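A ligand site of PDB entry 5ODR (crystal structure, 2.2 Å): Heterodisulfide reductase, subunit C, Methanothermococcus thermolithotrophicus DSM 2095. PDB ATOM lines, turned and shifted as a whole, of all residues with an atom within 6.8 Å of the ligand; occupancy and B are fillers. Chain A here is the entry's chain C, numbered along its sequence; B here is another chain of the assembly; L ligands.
CA of Gln 36 touches S1 of the ligand, at 3.6 Å.
CB of Thr 39 touches S3 of the ligand, at 3.7 Å.
Arg 55 touches the ligand (CG to S1, 3.8 Å).
Pro 88 touches the ligand.
Arg 89 touches the ligand.
Val 91 touches the ligand.
CG2 of Val 93 touches S2 of the ligand (3.5 Å).
Hydrophobic or aromatic side chains that line the ligand: Tyr 35, Pro 88, Val 91 and Val 93.
13 residues have an atom within 4 Å of the ligand: Cys 34, Tyr 35, Gln 36, Cys 37, Gly 38, Thr 39, Cys 40, Arg 55, Cys 87, Pro 88, Arg 89, Val 91 and Val 93.
The nearest printed residue that does not touch the ligand is Ile 58 (4.3 Å).
The side-chain sulfur of Met 428 of chain B lies close to the side-chain hydroxyl of Tyr 35, 3.7 Å away.
The guanidinium group (NH1) of Arg 456 of chain B is in hydrogen-bond range of the side-chain hydroxyl (OG1) of Thr 39, 3.1 Å away.
The side-chain sulfur (SG) of Cys 87 sits close to the backbone NH (N) of Val 91 (3.3 Å).
The side-chain sulfur (SG) of Cys 37 sits close to the side-chain hydroxyl (OG1) of Thr 39 (3.3 Å).
The side-chain hydroxyl (OG1) of Thr 41 is in hydrogen-bond range of the backbone NH (N) of Arg 55 (3.1 Å).
The side-chain sulfur (SG) of Cys 87 lies close to the backbone NH (N) of Asp 90, 3.7 Å away.
The side-chain sulfur of Cys 87 lies close to the backbone NH of Arg 89, at 3.3 Å.
O of Cys 37 sits at hydrogen-bond distance from N of Arg 456 of chain B (3.0 Å).
The side-chain sulfur of Cys 34 binds an iron atom (FE3) of the ligand (2.3 Å).
The backbone NH (N) of Tyr 35 sits close to a sulfur (S4) of the ligand, at 3.4 Å.
An iron atom (FE4) of the ligand is bound by the side-chain sulfur (SG) of Cys 40.
An iron atom (FE1) of the ligand is bound by the side-chain sulfur of Cys 87 (2.2 Å).
N of Gly 38 sits close to S1 of the ligand, 3.4 Å away.
The side-chain sulfur (SG) of Cys 37 binds an iron atom (FE2) of the ligand.
N of Cys 37 sits close to S1 of the ligand (3.3 Å).
The backbone NH (N) of Cys 40 lies close to a sulfur (S3) of the ligand (3.5 Å).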
ATOM      1  N   LEU A  31      -2.865 -23.453  -8.253  1.00  0.00           N
ATOM      2  CA  LEU A  31      -1.652 -24.272  -8.120  1.00  0.00           C
ATOM      3  C   LEU A  31      -1.603 -25.360  -9.197  1.00  0.00           C
ATOM      4  O   LEU A  31      -0.523 -25.810  -9.555  1.00  0.00           O
ATOM      5  CB  LEU A  31      -1.485 -24.875  -6.701  1.00  0.00           C
ATOM      6  CG  LEU A  31      -2.407 -26.023  -6.289  1.00  0.00           C
ATOM      7  CD1 LEU A  31      -1.849 -27.365  -6.722  1.00  0.00           C
ATOM      8  CD2 LEU A  31      -2.537 -26.084  -4.790  1.00  0.00           C
ATOM      9  N   ALA A  33      -2.445 -24.922 -12.336  1.00  0.00           N
ATOM     10  CA  ALA A  33      -2.048 -24.297 -13.607  1.00  0.00           C
ATOM     11  C   ALA A  33      -0.528 -24.169 -13.747  1.00  0.00           C
ATOM     12  O   ALA A  33      -0.062 -23.783 -14.817  1.00  0.00           O
ATOM     13  CB  ALA A  33      -2.678 -22.906 -13.719  1.00  0.00           C
ATOM     14  N   CYS A  34       0.245 -24.454 -12.694  1.00  0.00           N
ATOM     15  CA  CYS A  34       1.700 -24.333 -12.756  1.00  0.00           C
ATOM     16  C   CYS A  34       2.350 -25.211 -13.821  1.00  0.00           C
ATOM     17  O   CYS A  34       2.116 -26.419 -13.818  1.00  0.00           O
ATOM     18  CB  CYS A  34       2.319 -24.603 -11.389  1.00  0.00           C
ATOM     19  SG  CYS A  34       4.124 -24.750 -11.408  1.00  0.00           S
ATOM     20  N   TYR A  35       3.182 -24.626 -14.707  1.00  0.00           N
ATOM     21  CA  TYR A  35       3.859 -25.436 -15.722  1.00  0.00           C
ATOM     22  C   TYR A  35       5.388 -25.568 -15.456  1.00  0.00           C
ATOM     23  O   TYR A  35       6.173 -25.793 -16.382  1.00  0.00           O
ATOM     24  CB  TYR A  35       3.513 -25.056 -17.182  1.00  0.00           C
ATOM     25  CG  TYR A  35       3.723 -23.636 -17.645  1.00  0.00           C
ATOM     26  CD1 TYR A  35       4.514 -22.758 -16.922  1.00  0.00           C
ATOM     27  CD2 TYR A  35       3.160 -23.186 -18.833  1.00  0.00           C
ATOM     28  CE1 TYR A  35       4.711 -21.445 -17.359  1.00  0.00           C
ATOM     29  CE2 TYR A  35       3.361 -21.886 -19.279  1.00  0.00           C
ATOM     30  CZ  TYR A  35       4.132 -21.016 -18.534  1.00  0.00           C
ATOM     31  OH  TYR A  35       4.325 -19.737 -18.985  1.00  0.00           O
ATOM     32  N   GLN A  36       5.801 -25.426 -14.189  1.00  0.00           N
ATOM     33  CA  GLN A  36       7.192 -25.559 -13.748  1.00  0.00           C
ATOM     34  C   GLN A  36       8.234 -24.795 -14.566  1.00  0.00           C
ATOM     35  O   GLN A  36       9.269 -25.356 -14.916  1.00  0.00           O
ATOM     36  CB  GLN A  36       7.544 -27.052 -13.715  1.00  0.00           C
ATOM     37  CG  GLN A  36       6.713 -27.842 -12.708  1.00  0.00           C
ATOM     38  CD  GLN A  36       7.300 -27.678 -11.326  1.00  0.00           C
ATOM     39  OE1 GLN A  36       8.425 -28.115 -11.063  1.00  0.00           O
ATOM     40  NE2 GLN A  36       6.588 -26.987 -10.444  1.00  0.00           N
ATOM     41  N   CYS A  37       7.982 -23.522 -14.854  1.00  0.00           N
ATOM     42  CA  CYS A  37       8.910 -22.712 -15.630  1.00  0.00           C
ATOM     43  C   CYS A  37      10.132 -22.236 -14.826  1.00  0.00           C
ATOM     44  O   CYS A  37      11.199 -22.023 -15.404  1.00  0.00           O
ATOM     45  CB  CYS A  37       8.180 -21.541 -16.272  1.00  0.00           C
ATOM     46  SG  CYS A  37       7.632 -20.276 -15.102  1.00  0.00           S
ATOM     47  N   GLY A  38       9.968 -22.066 -13.520  1.00  0.00           N
ATOM     48  CA  GLY A  38      11.047 -21.622 -12.644  1.00  0.00           C
ATOM     49  C   GLY A  38      11.149 -20.113 -12.428  1.00  0.00           C
ATOM     50  O   GLY A  38      12.049 -19.659 -11.713  1.00  0.00           O
ATOM     51  N   THR A  39      10.249 -19.317 -13.041  1.00  0.00           N
ATOM     52  CA  THR A  39      10.252 -17.849 -12.900  1.00  0.00           C
ATOM     53  C   THR A  39      10.121 -17.455 -11.427  1.00  0.00           C
ATOM     54  O   THR A  39      10.730 -16.477 -11.000  1.00  0.00           O
ATOM     55  CB  THR A  39       9.121 -17.230 -13.739  1.00  0.00           C
ATOM     56  OG1 THR A  39       9.407 -17.438 -15.116  1.00  0.00           O
ATOM     57  CG2 THR A  39       8.924 -15.743 -13.487  1.00  0.00           C
ATOM     58  N   CYS A  40       9.331 -18.208 -10.646  1.00  0.00           N
ATOM     59  CA  CYS A  40       9.130 -17.929  -9.222  1.00  0.00           C
ATOM     60  C   CYS A  40      10.442 -18.122  -8.440  1.00  0.00           C
ATOM     61  O   CYS A  40      10.779 -17.291  -7.605  1.00  0.00           O
ATOM     62  CB  CYS A  40       8.019 -18.819  -8.657  1.00  0.00           C
ATOM     63  SG  CYS A  40       8.184 -20.565  -9.099  1.00  0.00           S
ATOM     64  N   THR A  41      11.176 -19.202  -8.730  1.00  0.00           N
ATOM     65  CA  THR A  41      12.440 -19.488  -8.053  1.00  0.00           C
ATOM     66  C   THR A  41      13.486 -18.422  -8.345  1.00  0.00           C
ATOM     67  O   THR A  41      14.179 -17.973  -7.433  1.00  0.00           O
ATOM     68  CB  THR A  41      12.985 -20.842  -8.493  1.00  0.00           C
ATOM     69  OG1 THR A  41      11.936 -21.813  -8.426  1.00  0.00           O
ATOM     70  CG2 THR A  41      14.171 -21.294  -7.645  1.00  0.00           C
ATOM     71  N   THR A  54      11.159 -22.204  -4.811  1.00  0.00           N
ATOM     72  CA  THR A  54       9.708 -21.999  -4.911  1.00  0.00           C
ATOM     73  C   THR A  54       9.024 -22.979  -5.839  1.00  0.00           C
ATOM     74  O   THR A  54       7.992 -23.531  -5.485  1.00  0.00           O
ATOM     75  CB  THR A  54       9.413 -20.568  -5.354  1.00  0.00           C
ATOM     76  OG1 THR A  54      10.302 -19.664  -4.693  1.00  0.00           O
ATOM     77  CG2 THR A  54       7.957 -20.181  -5.081  1.00  0.00           C
ATOM     78  N   ARG A  55       9.598 -23.217  -7.021  1.00  0.00           N
ATOM     79  CA  ARG A  55       9.037 -24.137  -8.008  1.00  0.00           C
ATOM     80  C   ARG A  55       8.893 -25.550  -7.455  1.00  0.00           C
ATOM     81  O   ARG A  55       7.870 -26.190  -7.684  1.00  0.00           O
ATOM     82  CB  ARG A  55       9.902 -24.152  -9.272  1.00  0.00           C
ATOM     83  CG  ARG A  55       9.384 -25.069 -10.371  1.00  0.00           C
ATOM     84  CD  ARG A  55      10.395 -25.283 -11.483  1.00  0.00           C
ATOM     85  NE  ARG A  55      11.728 -25.607 -10.974  1.00  0.00           N
ATOM     86  CZ  ARG A  55      12.137 -26.821 -10.613  1.00  0.00           C
ATOM     87  NH1 ARG A  55      13.357 -27.016 -10.160  1.00  0.00           N
ATOM     88  NH2 ARG A  55      11.300 -27.852 -10.685  1.00  0.00           N
ATOM     89  N   ILE A  58       5.819 -26.194  -5.280  1.00  0.00           N
ATOM     90  CA  ILE A  58       4.612 -26.388  -6.073  1.00  0.00           C
ATOM     91  C   ILE A  58       4.653 -27.802  -6.675  1.00  0.00           C
ATOM     92  O   ILE A  58       3.626 -28.478  -6.716  1.00  0.00           O
ATOM     93  CB  ILE A  58       4.448 -25.316  -7.187  1.00  0.00           C
ATOM     94  CG1 ILE A  58       4.490 -23.869  -6.632  1.00  0.00           C
ATOM     95  CG2 ILE A  58       3.155 -25.555  -7.991  1.00  0.00           C
ATOM     96  CD1 ILE A  58       3.341 -23.476  -5.735  1.00  0.00           C
ATOM     97  N   CYS A  83       6.947 -13.495  -7.009  1.00  0.00           N
ATOM     98  CA  CYS A  83       6.623 -14.660  -7.842  1.00  0.00           C
ATOM     99  C   CYS A  83       5.178 -14.529  -8.347  1.00  0.00           C
ATOM    100  O   CYS A  83       4.891 -14.832  -9.495  1.00  0.00           O
ATOM    101  CB  CYS A  83       6.820 -15.953  -7.053  1.00  0.00           C
ATOM    102  SG  CYS A  83       5.946 -15.987  -5.456  1.00  0.00           S
ATOM    103  N   ARG A  86       5.051 -12.048 -11.233  1.00  0.00           N
ATOM    104  CA  ARG A  86       5.679 -12.514 -12.460  1.00  0.00           C
ATOM    105  C   ARG A  86       5.217 -13.862 -13.007  1.00  0.00           C
ATOM    106  O   ARG A  86       5.641 -14.224 -14.102  1.00  0.00           O
ATOM    107  CB  ARG A  86       7.198 -12.557 -12.254  1.00  0.00           C
ATOM    108  CG  ARG A  86       7.795 -11.190 -11.962  1.00  0.00           C
ATOM    109  CD  ARG A  86       9.246 -11.315 -11.591  1.00  0.00           C
ATOM    110  NE  ARG A  86       9.842 -10.020 -11.278  1.00  0.00           N
ATOM    111  CZ  ARG A  86      11.047  -9.864 -10.748  1.00  0.00           C
ATOM    112  NH1 ARG A  86      11.797 -10.921 -10.466  1.00  0.00           N
ATOM    113  NH2 ARG A  86      11.520  -8.651 -10.501  1.00  0.00           N
ATOM    114  N   CYS A  87       4.385 -14.618 -12.282  1.00  0.00           N
ATOM    115  CA  CYS A  87       3.974 -15.920 -12.814  1.00  0.00           C
ATOM    116  C   CYS A  87       3.205 -15.801 -14.127  1.00  0.00           C
ATOM    117  O   CYS A  87       2.159 -15.164 -14.177  1.00  0.00           O
ATOM    118  CB  CYS A  87       3.195 -16.733 -11.803  1.00  0.00           C
ATOM    119  SG  CYS A  87       2.682 -18.352 -12.427  1.00  0.00           S
ATOM    120  N   PRO A  88       3.705 -16.430 -15.209  1.00  0.00           N
ATOM    121  CA  PRO A  88       2.992 -16.358 -16.483  1.00  0.00           C
ATOM    122  C   PRO A  88       1.750 -17.235 -16.538  1.00  0.00           C
ATOM    123  O   PRO A  88       0.942 -17.075 -17.465  1.00  0.00           O
ATOM    124  CB  PRO A  88       4.048 -16.835 -17.474  1.00  0.00           C
ATOM    125  CG  PRO A  88       4.852 -17.803 -16.700  1.00  0.00           C
ATOM    126  CD  PRO A  88       4.937 -17.238 -15.325  1.00  0.00           C
ATOM    127  N   ARG A  89       1.567 -18.155 -15.567  1.00  0.00           N
ATOM    128  CA  ARG A  89       0.394 -19.040 -15.541  1.00  0.00           C
ATOM    129  C   ARG A  89      -0.657 -18.594 -14.503  1.00  0.00           C
ATOM    130  O   ARG A  89      -1.604 -19.337 -14.232  1.00  0.00           O
ATOM    131  CB  ARG A  89       0.828 -20.497 -15.308  1.00  0.00           C
ATOM    132  CG  ARG A  89       0.985 -21.276 -16.594  1.00  0.00           C
ATOM    133  CD  ARG A  89      -0.354 -21.548 -17.253  1.00  0.00           C
ATOM    134  NE  ARG A  89      -0.224 -22.314 -18.485  1.00  0.00           N
ATOM    135  CZ  ARG A  89      -0.218 -23.643 -18.563  1.00  0.00           C
ATOM    136  NH1 ARG A  89      -0.334 -24.381 -17.463  1.00  0.00           N
ATOM    137  NH2 ARG A  89      -0.102 -24.249 -19.732  1.00  0.00           N
ATOM    138  N   ASP A  90      -0.509 -17.379 -13.940  1.00  0.00           N
ATOM    139  CA  ASP A  90      -1.439 -16.816 -12.949  1.00  0.00           C
ATOM    140  C   ASP A  90      -1.543 -17.641 -11.653  1.00  0.00           C
ATOM    141  O   ASP A  90      -2.595 -17.673 -11.018  1.00  0.00           O
ATOM    142  CB  ASP A  90      -2.838 -16.576 -13.573  1.00  0.00           C
ATOM    143  CG  ASP A  90      -3.071 -15.160 -14.075  1.00  0.00           C
ATOM    144  OD1 ASP A  90      -2.323 -14.244 -13.679  1.00  0.00           O
ATOM    145  OD2 ASP A  90      -4.028 -14.970 -14.865  1.00  0.00           O
ATOM    146  N   VAL A  91      -0.449 -18.275 -11.252  1.00  0.00           N
ATOM    147  CA  VAL A  91      -0.441 -19.081 -10.032  1.00  0.00           C
ATOM    148  C   VAL A  91      -0.347 -18.096  -8.860  1.00  0.00           C
ATOM    149  O   VAL A  91       0.598 -17.310  -8.814  1.00  0.00           O
ATOM    150  CB  VAL A  91       0.715 -20.103 -10.034  1.00  0.00           C
ATOM    151  CG1 VAL A  91       0.724 -20.940  -8.758  1.00  0.00           C
ATOM    152  CG2 VAL A  91       0.635 -21.008 -11.266  1.00  0.00           C
ATOM    153  N   LYS A  92      -1.313 -18.145  -7.932  1.00  0.00           N
ATOM    154  CA  LYS A  92      -1.319 -17.255  -6.768  1.00  0.00           C
ATOM    155  C   LYS A  92      -0.388 -17.935  -5.752  1.00  0.00           C
ATOM    156  O   LYS A  92      -0.825 -18.414  -4.704  1.00  0.00           O
ATOM    157  CB  LYS A  92      -2.753 -17.079  -6.227  1.00  0.00           C
ATOM    158  CG  LYS A  92      -3.787 -16.688  -7.301  1.00  0.00           C
ATOM    159  CD  LYS A  92      -3.566 -15.278  -7.848  1.00  0.00           C
ATOM    160  CE  LYS A  92      -4.652 -14.833  -8.814  1.00  0.00           C
ATOM    161  NZ  LYS A  92      -4.573 -15.493 -10.149  1.00  0.00           N
ATOM    162  N   VAL A  93       0.899 -17.978  -6.097  1.00  0.00           N
ATOM    163  CA  VAL A  93       1.955 -18.633  -5.332  1.00  0.00           C
ATOM    164  C   VAL A  93       1.985 -18.260  -3.865  1.00  0.00           C
ATOM    165  O   VAL A  93       1.946 -19.140  -3.010  1.00  0.00           O
ATOM    166  CB  VAL A  93       3.367 -18.407  -5.956  1.00  0.00           C
ATOM    167  CG1 VAL A  93       4.414 -19.243  -5.232  1.00  0.00           C
ATOM    168  CG2 VAL A  93       3.398 -18.717  -7.457  1.00  0.00           C
ATOM    169  N   MET B 428      11.188 -23.468 -21.923  1.00  0.00           N
ATOM    170  CA  MET B 428      10.269 -24.225 -21.063  1.00  0.00           C
ATOM    171  C   MET B 428      10.035 -25.556 -21.785  1.00  0.00           C
ATOM    172  O   MET B 428      10.235 -26.626 -21.215  1.00  0.00           O
ATOM    173  CB  MET B 428       8.932 -23.478 -20.890  1.00  0.00           C
ATOM    174  CG  MET B 428       9.068 -22.240 -20.041  1.00  0.00           C
ATOM    175  SD  MET B 428       7.455 -21.554 -19.607  1.00  0.00           S
ATOM    176  CE  MET B 428       6.999 -20.818 -21.129  1.00  0.00           C
ATOM    177  N   ARG B 456      12.515 -20.476 -17.588  1.00  0.00           N
ATOM    178  CA  ARG B 456      12.047 -19.196 -18.102  1.00  0.00           C
ATOM    179  C   ARG B 456      12.686 -18.104 -17.241  1.00  0.00           C
ATOM    180  O   ARG B 456      12.444 -18.061 -16.035  1.00  0.00           O
ATOM    181  CB  ARG B 456      10.536 -19.144 -18.033  1.00  0.00           C
ATOM    182  CG  ARG B 456       9.905 -17.914 -18.656  1.00  0.00           C
ATOM    183  CD  ARG B 456       8.410 -17.950 -18.399  1.00  0.00           C
ATOM    184  NE  ARG B 456       7.730 -16.752 -18.901  1.00  0.00           N
ATOM    185  CZ  ARG B 456       7.769 -15.561 -18.317  1.00  0.00           C
ATOM    186  NH1 ARG B 456       8.466 -15.376 -17.206  1.00  0.00           N
ATOM    187  NH2 ARG B 456       7.117 -14.540 -18.854  1.00  0.00           N
ATOM    188  N   GLU B 474      16.323 -19.926 -13.254  1.00  0.00           N
ATOM    189  CA  GLU B 474      16.598 -21.163 -12.547  1.00  0.00           C
ATOM    190  C   GLU B 474      16.812 -22.247 -13.572  1.00  0.00           C
ATOM    191  O   GLU B 474      15.993 -22.385 -14.487  1.00  0.00           O
ATOM    192  CB  GLU B 474      15.426 -21.583 -11.643  1.00  0.00           C
ATOM    193  CG  GLU B 474      15.743 -22.853 -10.869  1.00  0.00           C
ATOM    194  CD  GLU B 474      14.566 -23.626 -10.313  1.00  0.00           C
ATOM    195  OE1 GLU B 474      14.818 -24.640  -9.636  1.00  0.00           O
ATOM    196  OE2 GLU B 474      13.405 -23.256 -10.608  1.00  0.00           O
HETATM  197 FE1  LIG L   1       4.236 -19.876 -11.960  1.00  0.00          FE
HETATM  198 FE2  LIG L   1       6.295 -20.870 -13.295  1.00  0.00          FE
HETATM  199 FE3  LIG L   1       4.800 -22.592 -11.602  1.00  0.00          FE
HETATM  200 FE4  LIG L   1       6.520 -20.663 -10.567  1.00  0.00          FE
HETATM  201  S1  LIG L   1       7.069 -22.491 -11.849  1.00  0.00           S
HETATM  202  S2  LIG L   1       4.364 -21.051  -9.918  1.00  0.00           S
HETATM  203  S3  LIG L   1       6.250 -18.925 -12.042  1.00  0.00           S
HETATM  204  S4  LIG L   1       4.112 -21.565 -13.511  1.00  0.00           S
